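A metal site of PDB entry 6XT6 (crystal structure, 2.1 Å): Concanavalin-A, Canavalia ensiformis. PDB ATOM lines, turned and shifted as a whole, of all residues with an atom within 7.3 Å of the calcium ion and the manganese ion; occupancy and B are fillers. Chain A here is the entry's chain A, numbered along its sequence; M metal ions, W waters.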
ATOM      1  N   ALA A  89      24.725 -30.662 -24.132  1.00  0.00           N
ATOM      2  CA  ALA A  89      23.524 -29.806 -23.955  1.00  0.00           C
ATOM      3  C   ALA A  89      23.308 -29.608 -22.458  1.00  0.00           C
ATOM      4  O   ALA A  89      23.770 -30.450 -21.671  1.00  0.00           O
ATOM      5  CB  ALA A  89      22.334 -30.461 -24.611  1.00  0.00           C
ATOM      6  N   ASP A  90      22.639 -28.513 -22.038  1.00  0.00           N
ATOM      7  CA  ASP A  90      22.074 -27.467 -22.876  1.00  0.00           C
ATOM      8  C   ASP A  90      22.742 -26.107 -22.669  1.00  0.00           C
ATOM      9  O   ASP A  90      22.602 -25.235 -23.576  1.00  0.00           O
ATOM     10  CB  ASP A  90      20.583 -27.335 -22.619  1.00  0.00           C
ATOM     11  CG  ASP A  90      19.866 -28.377 -23.445  1.00  0.00           C
ATOM     12  OD1 ASP A  90      19.588 -28.096 -24.645  1.00  0.00           O
ATOM     13  OD2 ASP A  90      19.716 -29.501 -22.924  1.00  0.00           O
ATOM     14  N   GLY A  91      23.373 -25.919 -21.510  1.00  0.00           N
ATOM     15  CA  GLY A  91      24.298 -24.801 -21.281  1.00  0.00           C
ATOM     16  C   GLY A  91      24.214 -24.236 -19.876  1.00  0.00           C
ATOM     17  O   GLY A  91      23.558 -24.832 -19.001  1.00  0.00           O
ATOM     18  N   GLY A 109      16.583 -28.979 -20.032  1.00  0.00           N
ATOM     19  CA  GLY A 109      17.010 -28.889 -21.441  1.00  0.00           C
ATOM     20  C   GLY A 109      17.121 -27.446 -21.907  1.00  0.00           C
ATOM     21  O   GLY A 109      17.760 -26.650 -21.228  1.00  0.00           O
ATOM     22  N   ARG A 110      16.491 -27.140 -23.046  1.00  0.00           N
ATOM     23  CA  ARG A 110      16.621 -25.892 -23.850  1.00  0.00           C
ATOM     24  C   ARG A 110      16.221 -24.627 -23.074  1.00  0.00           C
ATOM     25  O   ARG A 110      16.657 -23.538 -23.487  1.00  0.00           O
ATOM     26  CB  ARG A 110      15.724 -26.013 -25.079  1.00  0.00           C
ATOM     27  CG  ARG A 110      14.377 -26.627 -24.722  1.00  0.00           C
ATOM     28  CD  ARG A 110      13.230 -26.248 -25.611  1.00  0.00           C
ATOM     29  NE  ARG A 110      13.287 -26.937 -26.874  1.00  0.00           N
ATOM     30  CZ  ARG A 110      12.217 -27.313 -27.566  1.00  0.00           C
ATOM     31  NH1 ARG A 110      11.004 -27.095 -27.104  1.00  0.00           N
ATOM     32  NH2 ARG A 110      12.385 -27.902 -28.740  1.00  0.00           N
ATOM     33  N   LEU A 111      15.424 -24.716 -22.003  1.00  0.00           N
ATOM     34  CA  LEU A 111      14.942 -23.530 -21.229  1.00  0.00           C
ATOM     35  C   LEU A 111      15.915 -23.172 -20.089  1.00  0.00           C
ATOM     36  O   LEU A 111      15.675 -22.155 -19.423  1.00  0.00           O
ATOM     37  CB  LEU A 111      13.522 -23.802 -20.721  1.00  0.00           C
ATOM     38  CG  LEU A 111      12.498 -24.138 -21.817  1.00  0.00           C
ATOM     39  CD1 LEU A 111      11.134 -24.464 -21.240  1.00  0.00           C
ATOM     40  CD2 LEU A 111      12.372 -22.996 -22.819  1.00  0.00           C
ATOM     41  N   LEU A 112      16.959 -23.970 -19.866  1.00  0.00           N
ATOM     42  CA  LEU A 112      18.165 -23.591 -19.063  1.00  0.00           C
ATOM     43  C   LEU A 112      17.830 -23.287 -17.587  1.00  0.00           C
ATOM     44  O   LEU A 112      18.668 -22.615 -16.945  1.00  0.00           O
ATOM     45  CB  LEU A 112      18.823 -22.373 -19.709  1.00  0.00           C
ATOM     46  CG  LEU A 112      19.291 -22.533 -21.148  1.00  0.00           C
ATOM     47  CD1 LEU A 112      19.907 -21.246 -21.655  1.00  0.00           C
ATOM     48  CD2 LEU A 112      20.274 -23.680 -21.294  1.00  0.00           C
ATOM     49  N   GLU A 142      23.356 -16.318 -21.583  1.00  0.00           N
ATOM     50  CA  GLU A 142      23.289 -17.782 -21.789  1.00  0.00           C
ATOM     51  C   GLU A 142      24.571 -18.189 -22.529  1.00  0.00           C
ATOM     52  O   GLU A 142      24.954 -17.508 -23.511  1.00  0.00           O
ATOM     53  CB  GLU A 142      21.962 -18.155 -22.462  1.00  0.00           C
ATOM     54  CG  GLU A 142      21.780 -17.663 -23.899  1.00  0.00           C
ATOM     55  CD  GLU A 142      20.672 -18.365 -24.716  1.00  0.00           C
ATOM     56  OE1 GLU A 142      19.494 -18.403 -24.273  1.00  0.00           O
ATOM     57  OE2 GLU A 142      20.997 -18.868 -25.817  1.00  0.00           O
ATOM     58  N   LEU A 143      25.253 -19.190 -21.974  1.00  0.00           N
ATOM     59  CA  LEU A 143      26.313 -19.967 -22.663  1.00  0.00           C
ATOM     60  C   LEU A 143      25.602 -21.197 -23.222  1.00  0.00           C
ATOM     61  O   LEU A 143      25.511 -22.200 -22.499  1.00  0.00           O
ATOM     62  CB  LEU A 143      27.429 -20.340 -21.686  1.00  0.00           C
ATOM     63  CG  LEU A 143      28.531 -19.297 -21.534  1.00  0.00           C
ATOM     64  CD1 LEU A 143      27.991 -17.959 -21.097  1.00  0.00           C
ATOM     65  CD2 LEU A 143      29.604 -19.790 -20.570  1.00  0.00           C
ATOM     66  N   ASP A 144      25.049 -21.051 -24.435  1.00  0.00           N
ATOM     67  CA  ASP A 144      24.155 -22.058 -25.058  1.00  0.00           C
ATOM     68  C   ASP A 144      24.991 -23.002 -25.923  1.00  0.00           C
ATOM     69  O   ASP A 144      25.470 -22.600 -27.008  1.00  0.00           O
ATOM     70  CB  ASP A 144      23.037 -21.371 -25.836  1.00  0.00           C
ATOM     71  CG  ASP A 144      21.981 -22.374 -26.252  1.00  0.00           C
ATOM     72  OD1 ASP A 144      22.295 -23.576 -26.297  1.00  0.00           O
ATOM     73  OD2 ASP A 144      20.835 -21.944 -26.504  1.00  0.00           O
ATOM     74  N   THR A 145      25.123 -24.249 -25.466  1.00  0.00           N
ATOM     75  CA  THR A 145      26.017 -25.291 -26.033  1.00  0.00           C
ATOM     76  C   THR A 145      25.320 -26.086 -27.139  1.00  0.00           C
ATOM     77  O   THR A 145      26.032 -26.782 -27.853  1.00  0.00           O
ATOM     78  CB  THR A 145      26.494 -26.265 -24.950  1.00  0.00           C
ATOM     79  OG1 THR A 145      25.367 -26.860 -24.306  1.00  0.00           O
ATOM     80  CG2 THR A 145      27.354 -25.581 -23.905  1.00  0.00           C
ATOM     81  N   TYR A 146      23.986 -25.984 -27.247  1.00  0.00           N
ATOM     82  CA  TYR A 146      23.157 -26.816 -28.141  1.00  0.00           C
ATOM     83  C   TYR A 146      22.150 -25.956 -28.908  1.00  0.00           C
ATOM     84  O   TYR A 146      21.244 -25.400 -28.316  1.00  0.00           O
ATOM     85  CB  TYR A 146      22.433 -27.897 -27.343  1.00  0.00           C
ATOM     86  CG  TYR A 146      21.734 -28.922 -28.194  1.00  0.00           C
ATOM     87  CD1 TYR A 146      20.422 -28.717 -28.590  1.00  0.00           C
ATOM     88  CD2 TYR A 146      22.391 -30.045 -28.654  1.00  0.00           C
ATOM     89  CE1 TYR A 146      19.753 -29.646 -29.362  1.00  0.00           C
ATOM     90  CE2 TYR A 146      21.740 -30.981 -29.450  1.00  0.00           C
ATOM     91  CZ  TYR A 146      20.413 -30.783 -29.794  1.00  0.00           C
ATOM     92  OH  TYR A 146      19.730 -31.656 -30.574  1.00  0.00           O
ATOM     93  N   PRO A 147      22.305 -25.836 -30.245  1.00  0.00           N
ATOM     94  CA  PRO A 147      21.420 -25.002 -31.057  1.00  0.00           C
ATOM     95  C   PRO A 147      20.058 -25.678 -31.253  1.00  0.00           C
ATOM     96  O   PRO A 147      20.022 -26.676 -31.943  1.00  0.00           O
ATOM     97  CB  PRO A 147      22.183 -24.834 -32.375  1.00  0.00           C
ATOM     98  CG  PRO A 147      23.002 -26.090 -32.506  1.00  0.00           C
ATOM     99  CD  PRO A 147      23.309 -26.510 -31.079  1.00  0.00           C
ATOM    100  N   ASN A 148      19.013 -25.118 -30.628  1.00  0.00           N
ATOM    101  CA  ASN A 148      17.577 -25.525 -30.806  1.00  0.00           C
ATOM    102  C   ASN A 148      16.884 -24.512 -31.736  1.00  0.00           C
ATOM    103  O   ASN A 148      16.411 -23.481 -31.246  1.00  0.00           O
ATOM    104  CB  ASN A 148      16.820 -25.569 -29.480  1.00  0.00           C
ATOM    105  CG  ASN A 148      17.521 -26.326 -28.366  1.00  0.00           C
ATOM    106  OD1 ASN A 148      18.391 -25.773 -27.676  1.00  0.00           O
ATOM    107  ND2 ASN A 148      17.157 -27.588 -28.168  1.00  0.00           N
ATOM    108  N   THR A 149      16.807 -24.782 -33.037  1.00  0.00           N
ATOM    109  CA  THR A 149      16.361 -23.762 -34.036  1.00  0.00           C
ATOM    110  C   THR A 149      14.858 -23.422 -33.858  1.00  0.00           C
ATOM    111  O   THR A 149      14.499 -22.304 -34.243  1.00  0.00           O
ATOM    112  CB  THR A 149      16.754 -24.148 -35.476  1.00  0.00           C
ATOM    113  OG1 THR A 149      16.273 -25.461 -35.744  1.00  0.00           O
ATOM    114  CG2 THR A 149      18.243 -24.115 -35.696  1.00  0.00           C
ATOM    115  N   ILE A 151      13.140 -22.859 -31.055  1.00  0.00           N
ATOM    116  CA  ILE A 151      12.980 -21.790 -30.034  1.00  0.00           C
ATOM    117  C   ILE A 151      13.946 -20.652 -30.354  1.00  0.00           C
ATOM    118  O   ILE A 151      14.199 -19.831 -29.470  1.00  0.00           O
ATOM    119  CB  ILE A 151      13.119 -22.354 -28.615  1.00  0.00           C
ATOM    120  CG1 ILE A 151      14.522 -22.889 -28.338  1.00  0.00           C
ATOM    121  CG2 ILE A 151      12.042 -23.393 -28.368  1.00  0.00           C
ATOM    122  CD1 ILE A 151      14.905 -22.865 -26.864  1.00  0.00           C
ATOM    123  N   GLY A 152      14.432 -20.573 -31.596  1.00  0.00           N
ATOM    124  CA  GLY A 152      15.037 -19.353 -32.158  1.00  0.00           C
ATOM    125  C   GLY A 152      16.528 -19.244 -31.883  1.00  0.00           C
ATOM    126  O   GLY A 152      17.061 -18.149 -32.025  1.00  0.00           O
ATOM    127  N   ASP A 153      17.204 -20.344 -31.550  1.00  0.00           N
ATOM    128  CA  ASP A 153      18.684 -20.364 -31.481  1.00  0.00           C
ATOM    129  C   ASP A 153      19.223 -20.227 -32.903  1.00  0.00           C
ATOM    130  O   ASP A 153      18.645 -20.793 -33.829  1.00  0.00           O
ATOM    131  CB  ASP A 153      19.184 -21.685 -30.888  1.00  0.00           C
ATOM    132  CG  ASP A 153      19.089 -21.809 -29.370  1.00  0.00           C
ATOM    133  OD1 ASP A 153      18.764 -20.804 -28.703  1.00  0.00           O
ATOM    134  OD2 ASP A 153      19.364 -22.929 -28.864  1.00  0.00           O
ATOM    135  N   PRO A 154      20.404 -19.592 -33.114  1.00  0.00           N
ATOM    136  CA  PRO A 154      21.138 -19.810 -34.363  1.00  0.00           C
ATOM    137  C   PRO A 154      21.662 -21.253 -34.388  1.00  0.00           C
ATOM    138  O   PRO A 154      21.594 -21.933 -33.380  1.00  0.00           O
ATOM    139  CB  PRO A 154      22.259 -18.768 -34.291  1.00  0.00           C
ATOM    140  CG  PRO A 154      22.505 -18.608 -32.819  1.00  0.00           C
ATOM    141  CD  PRO A 154      21.139 -18.742 -32.169  1.00  0.00           C
ATOM    142  N   TYR A 156      24.440 -22.794 -34.473  1.00  0.00           N
ATOM    143  CA  TYR A 156      25.734 -23.133 -33.815  1.00  0.00           C
ATOM    144  C   TYR A 156      25.604 -22.812 -32.313  1.00  0.00           C
ATOM    145  O   TYR A 156      24.687 -22.094 -31.890  1.00  0.00           O
ATOM    146  CB  TYR A 156      26.881 -22.354 -34.471  1.00  0.00           C
ATOM    147  CG  TYR A 156      26.516 -20.915 -34.769  1.00  0.00           C
ATOM    148  CD1 TYR A 156      26.331 -20.002 -33.747  1.00  0.00           C
ATOM    149  CD2 TYR A 156      26.289 -20.481 -36.065  1.00  0.00           C
ATOM    150  CE1 TYR A 156      25.957 -18.693 -33.995  1.00  0.00           C
ATOM    151  CE2 TYR A 156      25.905 -19.171 -36.344  1.00  0.00           C
ATOM    152  CZ  TYR A 156      25.742 -18.263 -35.299  1.00  0.00           C
ATOM    153  OH  TYR A 156      25.359 -16.968 -35.525  1.00  0.00           O
ATOM    154  N   HIS A 158      26.356 -20.756 -28.979  1.00  0.00           N
ATOM    155  CA  HIS A 158      26.320 -19.271 -28.962  1.00  0.00           C
ATOM    156  C   HIS A 158      26.254 -18.733 -27.540  1.00  0.00           C
ATOM    157  O   HIS A 158      25.875 -19.464 -26.614  1.00  0.00           O
ATOM    158  CB  HIS A 158      25.141 -18.785 -29.808  1.00  0.00           C
ATOM    159  CG  HIS A 158      23.845 -19.417 -29.388  1.00  0.00           C
ATOM    160  ND1 HIS A 158      23.513 -20.711 -29.732  1.00  0.00           N
ATOM    161  CD2 HIS A 158      22.832 -18.945 -28.637  1.00  0.00           C
ATOM    162  CE1 HIS A 158      22.337 -21.006 -29.233  1.00  0.00           C
ATOM    163  NE2 HIS A 158      21.896 -19.957 -28.553  1.00  0.00           N
ATOM    164  N   ILE A 159      26.659 -17.480 -27.374  1.00  0.00           N
ATOM    165  CA  ILE A 159      26.396 -16.679 -26.147  1.00  0.00           C
ATOM    166  C   ILE A 159      25.223 -15.764 -26.510  1.00  0.00           C
ATOM    167  O   ILE A 159      25.130 -15.313 -27.654  1.00  0.00           O
ATOM    168  CB  ILE A 159      27.670 -15.924 -25.693  1.00  0.00           C
ATOM    169  CG1 ILE A 159      28.072 -14.822 -26.657  1.00  0.00           C
ATOM    170  CG2 ILE A 159      28.798 -16.929 -25.517  1.00  0.00           C
ATOM    171  CD1 ILE A 159      29.394 -14.120 -26.304  1.00  0.00           C
ATOM    172  N   GLY A 160      24.312 -15.542 -25.596  1.00  0.00           N
ATOM    173  CA  GLY A 160      23.082 -14.817 -25.932  1.00  0.00           C
ATOM    174  C   GLY A 160      22.656 -13.944 -24.798  1.00  0.00           C
ATOM    175  O   GLY A 160      22.899 -14.356 -23.630  1.00  0.00           O
ATOM    176  N   ASP A 162      19.391 -12.530 -23.009  1.00  0.00           N
ATOM    177  CA  ASP A 162      17.956 -12.928 -22.857  1.00  0.00           C
ATOM    178  C   ASP A 162      17.252 -11.943 -21.911  1.00  0.00           C
ATOM    179  O   ASP A 162      17.653 -11.861 -20.729  1.00  0.00           O
ATOM    180  CB  ASP A 162      17.825 -14.359 -22.331  1.00  0.00           C
ATOM    181  CG  ASP A 162      18.508 -15.417 -23.188  1.00  0.00           C
ATOM    182  OD1 ASP A 162      18.929 -15.093 -24.309  1.00  0.00           O
ATOM    183  OD2 ASP A 162      18.607 -16.552 -22.721  1.00  0.00           O
ATOM    184  N   VAL A 166      13.612 -16.717 -23.365  1.00  0.00           N
ATOM    185  CA  VAL A 166      14.708 -17.645 -23.823  1.00  0.00           C
ATOM    186  C   VAL A 166      15.135 -17.279 -25.258  1.00  0.00           C
ATOM    187  O   VAL A 166      16.291 -17.590 -25.633  1.00  0.00           O
ATOM    188  CB  VAL A 166      14.255 -19.114 -23.718  1.00  0.00           C
ATOM    189  CG1 VAL A 166      13.301 -19.517 -24.825  1.00  0.00           C
ATOM    190  CG2 VAL A 166      15.441 -20.065 -23.643  1.00  0.00           C
ATOM    191  N   ARG A 167      14.264 -16.624 -26.049  1.00  0.00           N
ATOM    192  CA  ARG A 167      14.609 -16.220 -27.442  1.00  0.00           C
ATOM    193  C   ARG A 167      15.529 -14.996 -27.405  1.00  0.00           C
ATOM    194  O   ARG A 167      15.024 -13.875 -27.252  1.00  0.00           O
ATOM    195  CB  ARG A 167      13.343 -15.950 -28.245  1.00  0.00           C
ATOM    196  CG  ARG A 167      12.561 -17.211 -28.572  1.00  0.00           C
ATOM    197  CD  ARG A 167      11.178 -16.861 -29.067  1.00  0.00           C
ATOM    198  NE  ARG A 167      10.358 -18.056 -29.177  1.00  0.00           N
ATOM    199  CZ  ARG A 167      10.368 -18.902 -30.195  1.00  0.00           C
ATOM    200  NH1 ARG A 167      11.198 -18.717 -31.212  1.00  0.00           N
ATOM    201  NH2 ARG A 167       9.554 -19.945 -30.192  1.00  0.00           N
ATOM    202  N   SER A 168      16.832 -15.198 -27.529  1.00  0.00           N
ATOM    203  CA  SER A 168      17.870 -14.188 -27.230  1.00  0.00           C
ATOM    204  C   SER A 168      17.575 -12.954 -28.070  1.00  0.00           C
ATOM    205  O   SER A 168      17.120 -13.127 -29.190  1.00  0.00           O
ATOM    206  CB  SER A 168      19.250 -14.720 -27.479  1.00  0.00           C
ATOM    207  OG  SER A 168      19.425 -15.974 -26.823  1.00  0.00           O
ATOM    208  N   THR A 171      22.771 -12.560 -30.136  1.00  0.00           N
ATOM    209  CA  THR A 171      23.649 -13.744 -29.918  1.00  0.00           C
ATOM    210  C   THR A 171      24.975 -13.511 -30.628  1.00  0.00           C
ATOM    211  O   THR A 171      25.001 -12.670 -31.521  1.00  0.00           O
ATOM    212  CB  THR A 171      22.989 -15.021 -30.449  1.00  0.00           C
ATOM    213  OG1 THR A 171      22.908 -14.762 -31.845  1.00  0.00           O
ATOM    214  CG2 THR A 171      21.623 -15.290 -29.873  1.00  0.00           C
HETATM  215 CA    CA M   1      19.875 -24.076 -26.951  1.00  0.00          CA
HETATM  216 MN    MN M   2      20.192 -19.955 -27.225  1.00  0.00          MN
HETATM  217  O   HOH W   1      18.398 -22.827 -25.632  1.00  0.00           O
HETATM  218  O   HOH W   2      19.511 -18.297 -27.969  1.00  0.00           O
HETATM  219  O   HOH W   3      18.481 -20.028 -26.049  1.00  0.00           O
HETATM  220  O   HOH W   4      20.389 -25.450 -25.041  1.00  0.00           O
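Four residues have an atom within 4 Å of the manganese ion: Glu 142, Asp 144, Asp 153 and His 158.
Four residues have an atom within 4 Å of the calcium ion: Asp 144, Tyr 146, Asn 148 and Asp 153.
Along chain A the residues within 4 Å of the calcium ion span positions 144 to 153.
The manganese ion is bound by water W2 (1.9 Å), the side-chain carboxylate (OE2) of Glu 142 (2.0 Å), water W3 (2.1 Å), a ring nitrogen (NE2) of His 158 (2.2 Å), the side-chain carboxylate (OD2) of Asp 144 (2.2 Å) and the side-chain carboxylate (OD1) of Asp 153 (2.2 Å).
The backbone carbonyl oxygen (O) of Tyr 156 lies within hydrogen-bond range of a ring nitrogen (ND1) of His 158 (2.8 Å).
OE1 of Glu 142 sits close to OD2 of Asp 162 (2.6 Å).
The side-chain carboxylate (OE2) of Glu 142 lies close to the side-chain hydroxyl (OG) of Ser 168 (3.4 Å).
The backbone carbonyl oxygen of Gly 160 is in hydrogen-bond range of the backbone NH of Glu 142, at 2.9 Å.
Water W3 lies within hydrogen-bond range of OE1 of Glu 142 (2.6 Å) and O of Val 166 (3.3 Å).
The side-chain carboxylate (OD2) of Asp 153 is bound to the calcium ion.
Water W1 is bound to the calcium ion, at 2.3 Å.
O of Tyr 146 is bound to the calcium ion (2.3 Å).
OD1 of Asn 148 is bound to the calcium ion, at 2.4 Å.
The side-chain carboxylate (OD2) of Asp 144 is bound to the calcium ion (2.4 Å).
Water W4 binds the calcium ion, 2.4 Å away.
OD1 of Asp 144 is bound to the calcium ion, at 2.6 Å.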
